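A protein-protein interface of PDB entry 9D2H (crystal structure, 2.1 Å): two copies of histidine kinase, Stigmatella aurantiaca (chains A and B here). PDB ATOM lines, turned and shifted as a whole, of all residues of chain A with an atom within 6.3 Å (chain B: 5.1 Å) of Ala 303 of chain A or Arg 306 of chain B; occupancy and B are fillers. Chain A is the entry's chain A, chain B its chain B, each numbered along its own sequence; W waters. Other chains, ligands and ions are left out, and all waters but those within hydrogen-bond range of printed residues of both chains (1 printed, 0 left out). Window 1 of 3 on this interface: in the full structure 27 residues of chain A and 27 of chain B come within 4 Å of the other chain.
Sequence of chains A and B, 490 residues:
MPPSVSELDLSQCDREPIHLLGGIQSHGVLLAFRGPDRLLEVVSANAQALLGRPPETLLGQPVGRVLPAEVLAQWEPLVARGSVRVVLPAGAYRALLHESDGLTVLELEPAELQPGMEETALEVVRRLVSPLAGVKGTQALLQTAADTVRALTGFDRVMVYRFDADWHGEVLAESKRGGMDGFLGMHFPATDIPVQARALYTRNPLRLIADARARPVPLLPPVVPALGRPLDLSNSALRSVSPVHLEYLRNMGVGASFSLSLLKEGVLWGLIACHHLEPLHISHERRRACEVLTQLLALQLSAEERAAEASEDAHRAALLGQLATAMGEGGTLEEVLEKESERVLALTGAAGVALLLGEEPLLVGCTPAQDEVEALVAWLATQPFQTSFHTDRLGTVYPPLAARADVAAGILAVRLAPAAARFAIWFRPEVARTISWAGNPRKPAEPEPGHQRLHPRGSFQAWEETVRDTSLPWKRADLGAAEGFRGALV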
ATOM      1  N   ALA A 298      -0.492 -15.352 -11.874  1.00  0.00           N
ATOM      2  CA  ALA A 298      -1.482 -16.424 -11.892  1.00  0.00           C
ATOM      3  C   ALA A 298      -0.877 -17.715 -11.370  1.00  0.00           C
ATOM      4  O   ALA A 298      -1.477 -18.397 -10.533  1.00  0.00           O
ATOM      5  CB  ALA A 298      -2.031 -16.614 -13.308  1.00  0.00           C
ATOM      6  N   LEU A 299       0.341 -18.025 -11.817  1.00  0.00           N
ATOM      7  CA  LEU A 299       1.035 -19.247 -11.429  1.00  0.00           C
ATOM      8  C   LEU A 299       1.458 -19.219  -9.956  1.00  0.00           C
ATOM      9  O   LEU A 299       1.313 -20.222  -9.244  1.00  0.00           O
ATOM     10  CB  LEU A 299       2.234 -19.427 -12.360  1.00  0.00           C
ATOM     11  CG  LEU A 299       3.203 -20.589 -12.197  1.00  0.00           C
ATOM     12  CD1 LEU A 299       2.447 -21.898 -12.205  1.00  0.00           C
ATOM     13  CD2 LEU A 299       4.257 -20.548 -13.299  1.00  0.00           C
ATOM     14  N   GLN A 300       1.976 -18.074  -9.481  1.00  0.00           N
ATOM     15  CA  GLN A 300       2.275 -17.890  -8.057  1.00  0.00           C
ATOM     16  C   GLN A 300       1.033 -18.038  -7.180  1.00  0.00           C
ATOM     17  O   GLN A 300       1.137 -18.495  -6.032  1.00  0.00           O
ATOM     18  CB  GLN A 300       2.885 -16.509  -7.811  1.00  0.00           C
ATOM     19  CG  GLN A 300       4.170 -16.227  -8.531  1.00  0.00           C
ATOM     20  CD  GLN A 300       5.364 -16.453  -7.646  1.00  0.00           C
ATOM     21  OE1 GLN A 300       5.621 -17.574  -7.205  1.00  0.00           O
ATOM     22  NE2 GLN A 300       6.090 -15.386  -7.355  1.00  0.00           N
ATOM     23  N   LEU A 301      -0.141 -17.629  -7.676  1.00  0.00           N
ATOM     24  CA  LEU A 301      -1.346 -17.756  -6.864  1.00  0.00           C
ATOM     25  C   LEU A 301      -1.840 -19.193  -6.787  1.00  0.00           C
ATOM     26  O   LEU A 301      -2.372 -19.597  -5.747  1.00  0.00           O
ATOM     27  CB  LEU A 301      -2.458 -16.864  -7.408  1.00  0.00           C
ATOM     28  CG  LEU A 301      -2.263 -15.352  -7.341  1.00  0.00           C
ATOM     29  CD1 LEU A 301      -3.567 -14.698  -7.747  1.00  0.00           C
ATOM     30  CD2 LEU A 301      -1.839 -14.898  -5.945  1.00  0.00           C
ATOM     31  N   SER A 302      -1.682 -19.976  -7.860  1.00  0.00           N
ATOM     32  CA  SER A 302      -2.177 -21.351  -7.829  1.00  0.00           C
ATOM     33  C   SER A 302      -1.373 -22.207  -6.863  1.00  0.00           C
ATOM     34  O   SER A 302      -1.945 -23.014  -6.120  1.00  0.00           O
ATOM     35  CB  SER A 302      -2.144 -21.963  -9.225  1.00  0.00           C
ATOM     36  OG  SER A 302      -3.025 -21.270 -10.079  1.00  0.00           O
ATOM     37  N   ALA A 303      -0.045 -22.038  -6.854  1.00  0.00           N
ATOM     38  CA  ALA A 303       0.799 -22.828  -5.960  1.00  0.00           C
ATOM     39  C   ALA A 303       0.583 -22.431  -4.504  1.00  0.00           C
ATOM     40  O   ALA A 303       0.485 -23.297  -3.628  1.00  0.00           O
ATOM     41  CB  ALA A 303       2.269 -22.669  -6.349  1.00  0.00           C
ATOM     42  N   GLU A 304       0.526 -21.128  -4.227  1.00  0.00           N
ATOM     43  CA  GLU A 304       0.199 -20.665  -2.885  1.00  0.00           C
ATOM     44  C   GLU A 304      -1.162 -21.174  -2.448  1.00  0.00           C
ATOM     45  O   GLU A 304      -1.323 -21.638  -1.315  1.00  0.00           O
ATOM     46  CB  GLU A 304       0.226 -19.141  -2.840  1.00  0.00           C
ATOM     47  CG  GLU A 304       1.550 -18.577  -2.425  1.00  0.00           C
ATOM     48  CD  GLU A 304       1.862 -18.878  -0.971  1.00  0.00           C
ATOM     49  OE1 GLU A 304       1.114 -18.372  -0.101  1.00  0.00           O
ATOM     50  OE2 GLU A 304       2.842 -19.623  -0.701  1.00  0.00           O
ATOM     51  N   GLU A 305      -2.158 -21.097  -3.334  1.00  0.00           N
ATOM     52  CA  GLU A 305      -3.514 -21.451  -2.935  1.00  0.00           C
ATOM     53  C   GLU A 305      -3.632 -22.944  -2.666  1.00  0.00           C
ATOM     54  O   GLU A 305      -4.174 -23.361  -1.634  1.00  0.00           O
ATOM     55  CB  GLU A 305      -4.516 -21.016  -3.997  1.00  0.00           C
ATOM     56  CG  GLU A 305      -5.857 -20.655  -3.402  1.00  0.00           C
ATOM     57  CD  GLU A 305      -6.931 -20.449  -4.445  1.00  0.00           C
ATOM     58  OE1 GLU A 305      -6.698 -19.669  -5.406  1.00  0.00           O
ATOM     59  OE2 GLU A 305      -8.008 -21.078  -4.295  1.00  0.00           O
ATOM     60  N   ARG A 306      -3.120 -23.771  -3.571  1.00  0.00           N
ATOM     61  CA  ARG A 306      -3.158 -25.194  -3.281  1.00  0.00           C
ATOM     62  C   ARG A 306      -2.246 -25.547  -2.112  1.00  0.00           C
ATOM     63  O   ARG A 306      -2.464 -26.586  -1.471  1.00  0.00           O
ATOM     64  CB  ARG A 306      -2.821 -25.995  -4.541  1.00  0.00           C
ATOM     65  CG  ARG A 306      -3.941 -25.905  -5.576  1.00  0.00           C
ATOM     66  CD  ARG A 306      -3.750 -26.837  -6.757  1.00  0.00           C
ATOM     67  NE  ARG A 306      -2.868 -26.261  -7.768  1.00  0.00           N
ATOM     68  CZ  ARG A 306      -3.209 -26.038  -9.032  1.00  0.00           C
ATOM     69  NH1 ARG A 306      -4.424 -26.321  -9.484  1.00  0.00           N
ATOM     70  NH2 ARG A 306      -2.304 -25.531  -9.867  1.00  0.00           N
ATOM     71  N   ALA A 307      -1.279 -24.678  -1.774  1.00  0.00           N
ATOM     72  CA  ALA A 307      -0.491 -24.888  -0.562  1.00  0.00           C
ATOM     73  C   ALA A 307      -1.334 -24.644   0.686  1.00  0.00           C
ATOM     74  O   ALA A 307      -1.311 -25.451   1.627  1.00  0.00           O
ATOM     75  CB  ALA A 307       0.744 -23.992  -0.560  1.00  0.00           C
ATOM     76  N   ALA A 308      -2.096 -23.548   0.699  1.00  0.00           N
ATOM     77  CA  ALA A 308      -2.945 -23.228   1.841  1.00  0.00           C
ATOM     78  C   ALA A 308      -3.976 -24.321   2.089  1.00  0.00           C
ATOM     79  O   ALA A 308      -4.131 -24.800   3.219  1.00  0.00           O
ATOM     80  CB  ALA A 308      -3.641 -21.888   1.613  1.00  0.00           C
ATOM     81  N   ALA A 310      -3.970 -27.430   1.264  1.00  0.00           N
ATOM     82  CA  ALA A 310      -3.385 -28.678   1.752  1.00  0.00           C
ATOM     83  C   ALA A 310      -2.994 -28.552   3.216  1.00  0.00           C
ATOM     84  O   ALA A 310      -3.161 -29.496   3.995  1.00  0.00           O
ATOM     85  CB  ALA A 310      -2.176 -29.084   0.902  1.00  0.00           C
ATOM     86  N   GLU B 265      11.354 -26.122  -2.829  1.00  0.00           N
ATOM     87  CA  GLU B 265      10.838 -25.401  -1.661  1.00  0.00           C
ATOM     88  C   GLU B 265      11.930 -25.345  -0.603  1.00  0.00           C
ATOM     89  O   GLU B 265      11.789 -25.871   0.500  1.00  0.00           O
ATOM     90  CB  GLU B 265       9.570 -26.038  -1.092  1.00  0.00           C
ATOM     91  CG  GLU B 265       8.355 -25.819  -1.962  1.00  0.00           C
ATOM     92  CD  GLU B 265       7.215 -26.733  -1.584  1.00  0.00           C
ATOM     93  OE1 GLU B 265       6.910 -26.820  -0.371  1.00  0.00           O
ATOM     94  OE2 GLU B 265       6.637 -27.376  -2.497  1.00  0.00           O
ATOM     95  N   LEU B 299       8.907 -23.549  -9.889  1.00  0.00           N
ATOM     96  CA  LEU B 299       7.560 -23.094  -9.580  1.00  0.00           C
ATOM     97  C   LEU B 299       6.509 -23.946 -10.290  1.00  0.00           C
ATOM     98  O   LEU B 299       5.496 -24.324  -9.685  1.00  0.00           O
ATOM     99  CB  LEU B 299       7.446 -21.616  -9.965  1.00  0.00           C
ATOM    100  CG  LEU B 299       6.112 -20.873  -9.903  1.00  0.00           C
ATOM    101  CD1 LEU B 299       5.485 -20.979  -8.532  1.00  0.00           C
ATOM    102  CD2 LEU B 299       6.317 -19.429 -10.294  1.00  0.00           C
ATOM    103  N   LEU B 301       6.751 -27.034 -11.185  1.00  0.00           N
ATOM    104  CA  LEU B 301       6.711 -28.390 -10.657  1.00  0.00           C
ATOM    105  C   LEU B 301       6.024 -28.437  -9.300  1.00  0.00           C
ATOM    106  O   LEU B 301       5.310 -29.405  -9.000  1.00  0.00           O
ATOM    107  CB  LEU B 301       8.125 -28.959 -10.566  1.00  0.00           C
ATOM    108  CG  LEU B 301       8.819 -29.250 -11.896  1.00  0.00           C
ATOM    109  CD1 LEU B 301      10.298 -29.491 -11.655  1.00  0.00           C
ATOM    110  CD2 LEU B 301       8.181 -30.458 -12.603  1.00  0.00           C
ATOM    111  N   SER B 302       6.225 -27.415  -8.465  1.00  0.00           N
ATOM    112  CA  SER B 302       5.491 -27.370  -7.201  1.00  0.00           C
ATOM    113  C   SER B 302       3.988 -27.340  -7.450  1.00  0.00           C
ATOM    114  O   SER B 302       3.236 -28.131  -6.872  1.00  0.00           O
ATOM    115  CB  SER B 302       5.926 -26.163  -6.366  1.00  0.00           C
ATOM    116  OG  SER B 302       7.063 -26.486  -5.582  1.00  0.00           O
ATOM    117  N   ALA B 303       3.536 -26.455  -8.342  1.00  0.00           N
ATOM    118  CA  ALA B 303       2.104 -26.283  -8.538  1.00  0.00           C
ATOM    119  C   ALA B 303       1.454 -27.501  -9.192  1.00  0.00           C
ATOM    120  O   ALA B 303       0.268 -27.758  -8.960  1.00  0.00           O
ATOM    121  CB  ALA B 303       1.848 -25.025  -9.368  1.00  0.00           C
ATOM    122  N   GLU B 304       2.189 -28.247 -10.022  1.00  0.00           N
ATOM    123  CA  GLU B 304       1.630 -29.457 -10.615  1.00  0.00           C
ATOM    124  C   GLU B 304       1.662 -30.608  -9.630  1.00  0.00           C
ATOM    125  O   GLU B 304       0.715 -31.400  -9.566  1.00  0.00           O
ATOM    126  CB  GLU B 304       2.392 -29.847 -11.879  1.00  0.00           C
ATOM    127  CG  GLU B 304       1.958 -29.097 -13.135  1.00  0.00           C
ATOM    128  CD  GLU B 304       0.582 -29.516 -13.627  1.00  0.00           C
ATOM    129  OE1 GLU B 304       0.276 -30.735 -13.598  1.00  0.00           O
ATOM    130  OE2 GLU B 304      -0.192 -28.624 -14.043  1.00  0.00           O
ATOM    131  N   GLU B 305       2.746 -30.722  -8.865  1.00  0.00           N
ATOM    132  CA  GLU B 305       2.804 -31.739  -7.826  1.00  0.00           C
ATOM    133  C   GLU B 305       1.684 -31.535  -6.814  1.00  0.00           C
ATOM    134  O   GLU B 305       0.951 -32.475  -6.478  1.00  0.00           O
ATOM    135  CB  GLU B 305       4.173 -31.716  -7.145  1.00  0.00           C
ATOM    136  CG  GLU B 305       4.284 -32.616  -5.923  1.00  0.00           C
ATOM    137  CD  GLU B 305       5.725 -33.003  -5.611  1.00  0.00           C
ATOM    138  OE1 GLU B 305       6.613 -32.145  -5.792  1.00  0.00           O
ATOM    139  OE2 GLU B 305       5.967 -34.166  -5.202  1.00  0.00           O
ATOM    140  N   ARG B 306       1.510 -30.300  -6.341  1.00  0.00           N
ATOM    141  CA  ARG B 306       0.444 -30.044  -5.382  1.00  0.00           C
ATOM    142  C   ARG B 306      -0.929 -30.289  -5.998  1.00  0.00           C
ATOM    143  O   ARG B 306      -1.842 -30.745  -5.302  1.00  0.00           O
ATOM    144  CB  ARG B 306       0.562 -28.620  -4.822  1.00  0.00           C
ATOM    145  CG  ARG B 306       1.888 -28.357  -4.084  1.00  0.00           C
ATOM    146  CD  ARG B 306       1.707 -27.501  -2.831  1.00  0.00           C
ATOM    147  NE  ARG B 306       2.950 -26.871  -2.387  1.00  0.00           N
ATOM    148  CZ  ARG B 306       3.418 -25.713  -2.847  1.00  0.00           C
ATOM    149  NH1 ARG B 306       2.804 -25.047  -3.811  1.00  0.00           N
ATOM    150  NH2 ARG B 306       4.530 -25.203  -2.321  1.00  0.00           N
ATOM    151  N   ALA B 307      -1.093 -30.026  -7.304  1.00  0.00           N
ATOM    152  CA  ALA B 307      -2.372 -30.321  -7.950  1.00  0.00           C
ATOM    153  C   ALA B 307      -2.588 -31.821  -8.096  1.00  0.00           C
ATOM    154  O   ALA B 307      -3.716 -32.307  -7.980  1.00  0.00           O
ATOM    155  CB  ALA B 307      -2.458 -29.637  -9.312  1.00  0.00           C
ATOM    156  N   ALA B 308      -1.521 -32.571  -8.356  1.00  0.00           N
ATOM    157  CA  ALA B 308      -1.649 -34.015  -8.453  1.00  0.00           C
ATOM    158  C   ALA B 308      -2.059 -34.616  -7.117  1.00  0.00           C
ATOM    159  O   ALA B 308      -2.944 -35.477  -7.062  1.00  0.00           O
ATOM    160  CB  ALA B 308      -0.334 -34.621  -8.935  1.00  0.00           C
ATOM    161  N   GLU B 309      -1.433 -34.165  -6.030  1.00  0.00           N
ATOM    162  CA  GLU B 309      -1.713 -34.728  -4.713  1.00  0.00           C
ATOM    163  C   GLU B 309      -3.114 -34.373  -4.222  1.00  0.00           C
ATOM    164  O   GLU B 309      -3.737 -35.167  -3.506  1.00  0.00           O
ATOM    165  CB  GLU B 309      -0.655 -34.261  -3.722  1.00  0.00           C
ATOM    166  CG  GLU B 309       0.756 -34.586  -4.165  1.00  0.00           C
ATOM    167  CD  GLU B 309       1.724 -34.687  -3.004  1.00  0.00           C
ATOM    168  OE1 GLU B 309       1.694 -35.724  -2.304  1.00  0.00           O
ATOM    169  OE2 GLU B 309       2.510 -33.732  -2.790  1.00  0.00           O
ATOM    170  N   ALA B 310      -3.630 -33.204  -4.602  1.00  0.00           N
ATOM    171  CA  ALA B 310      -5.034 -32.894  -4.344  1.00  0.00           C
ATOM    172  C   ALA B 310      -5.968 -33.848  -5.092  1.00  0.00           C
ATOM    173  O   ALA B 310      -6.890 -34.425  -4.501  1.00  0.00           O
ATOM    174  CB  ALA B 310      -5.317 -31.446  -4.732  1.00  0.00           C
HETATM  175  O   HOH W   1      -2.039 -27.199 -12.617  1.00  0.00           O
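O of Ala 303 of chain A sits at hydrogen-bond distance from NH1 of Arg 306 of chain B.
The side-chain carboxylate (OE2) of Glu 265 of chain B lies within salt-bridge range of the guanidinium group (NH2) of Arg 306 of chain B.
Among the printed residues, merely in contact across the chains: Leu 299 of chain A with Leu 299 of chain B (3.7 Å), Gln 300 of chain A with Leu 299 of chain B (3.7 Å), Ala 303 of chain A with Ala 303 of chain B (3.9 Å), Arg 306 of chain A with Ala 303 of chain B (3.5 Å), Arg 306 of chain A with Ala 307 of chain B (3.7 Å) and Ala 307 of chain A with Arg 306 of chain B (3.9 Å).
Of the printed residues of chain B, Leu 299 of chain A touches Leu 299. Printed residues of chain B within 4 Å of Arg 306 of chain A: Ala 303 and Ala 307. Of the printed residues of chain A, Leu 299 of chain B touches Leu 299 (3.7 Å) and Gln 300 (3.7 Å). Of chain A, only Ala 303 and Ala 307 come within 4 Å of Arg 306 of chain B. The nearest residue of chain B that does not touch Ala 303 of chain A is Leu 299 of chain B (4.2 Å). The nearest residue of chain A that does not touch Arg 306 of chain B is Arg 306 of chain A (4.3 Å).
Printed residues of chain B that touch a printed residue of chain A: Leu 299, Ala 303, Arg 306 and Ala 307. Hydrophobic or aromatic side chains of chain B that line the printed part of chain A: Leu 299, Ala 303 and Ala 307. Printed residues of chain A that touch a printed residue of chain B: Leu 299, Gln 300, Ala 303, Arg 306 and Ala 307. Hydrophobic or aromatic side chains of chain A that line the printed part of chain B: Leu 299, Ala 303 and Ala 307. Among the printed residues, no Asp or Glu carboxylate lies within 4 Å of a Lys or Arg side-chain nitrogen of the other chain.
Leu 299 of chain B touches its own counterpart, Leu 299 of chain A. Ala 303 of chain A touches its own counterpart, Ala 303 of chain B. Ala 303 of chain A touches Arg 306 of chain B, and with the chains exchanged Arg 306 of chain A touches Ala 303 of chain B. Arg 306 of chain A touches Ala 307 of chain B, and with the chains exchanged Ala 307 of chain A touches Arg 306 of chain B.
Water W1 lies within hydrogen-bond range of OE2 of Glu 304 of chain B (2.7 Å) and NH2 of Arg 306 of chain A (3.2 Å).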
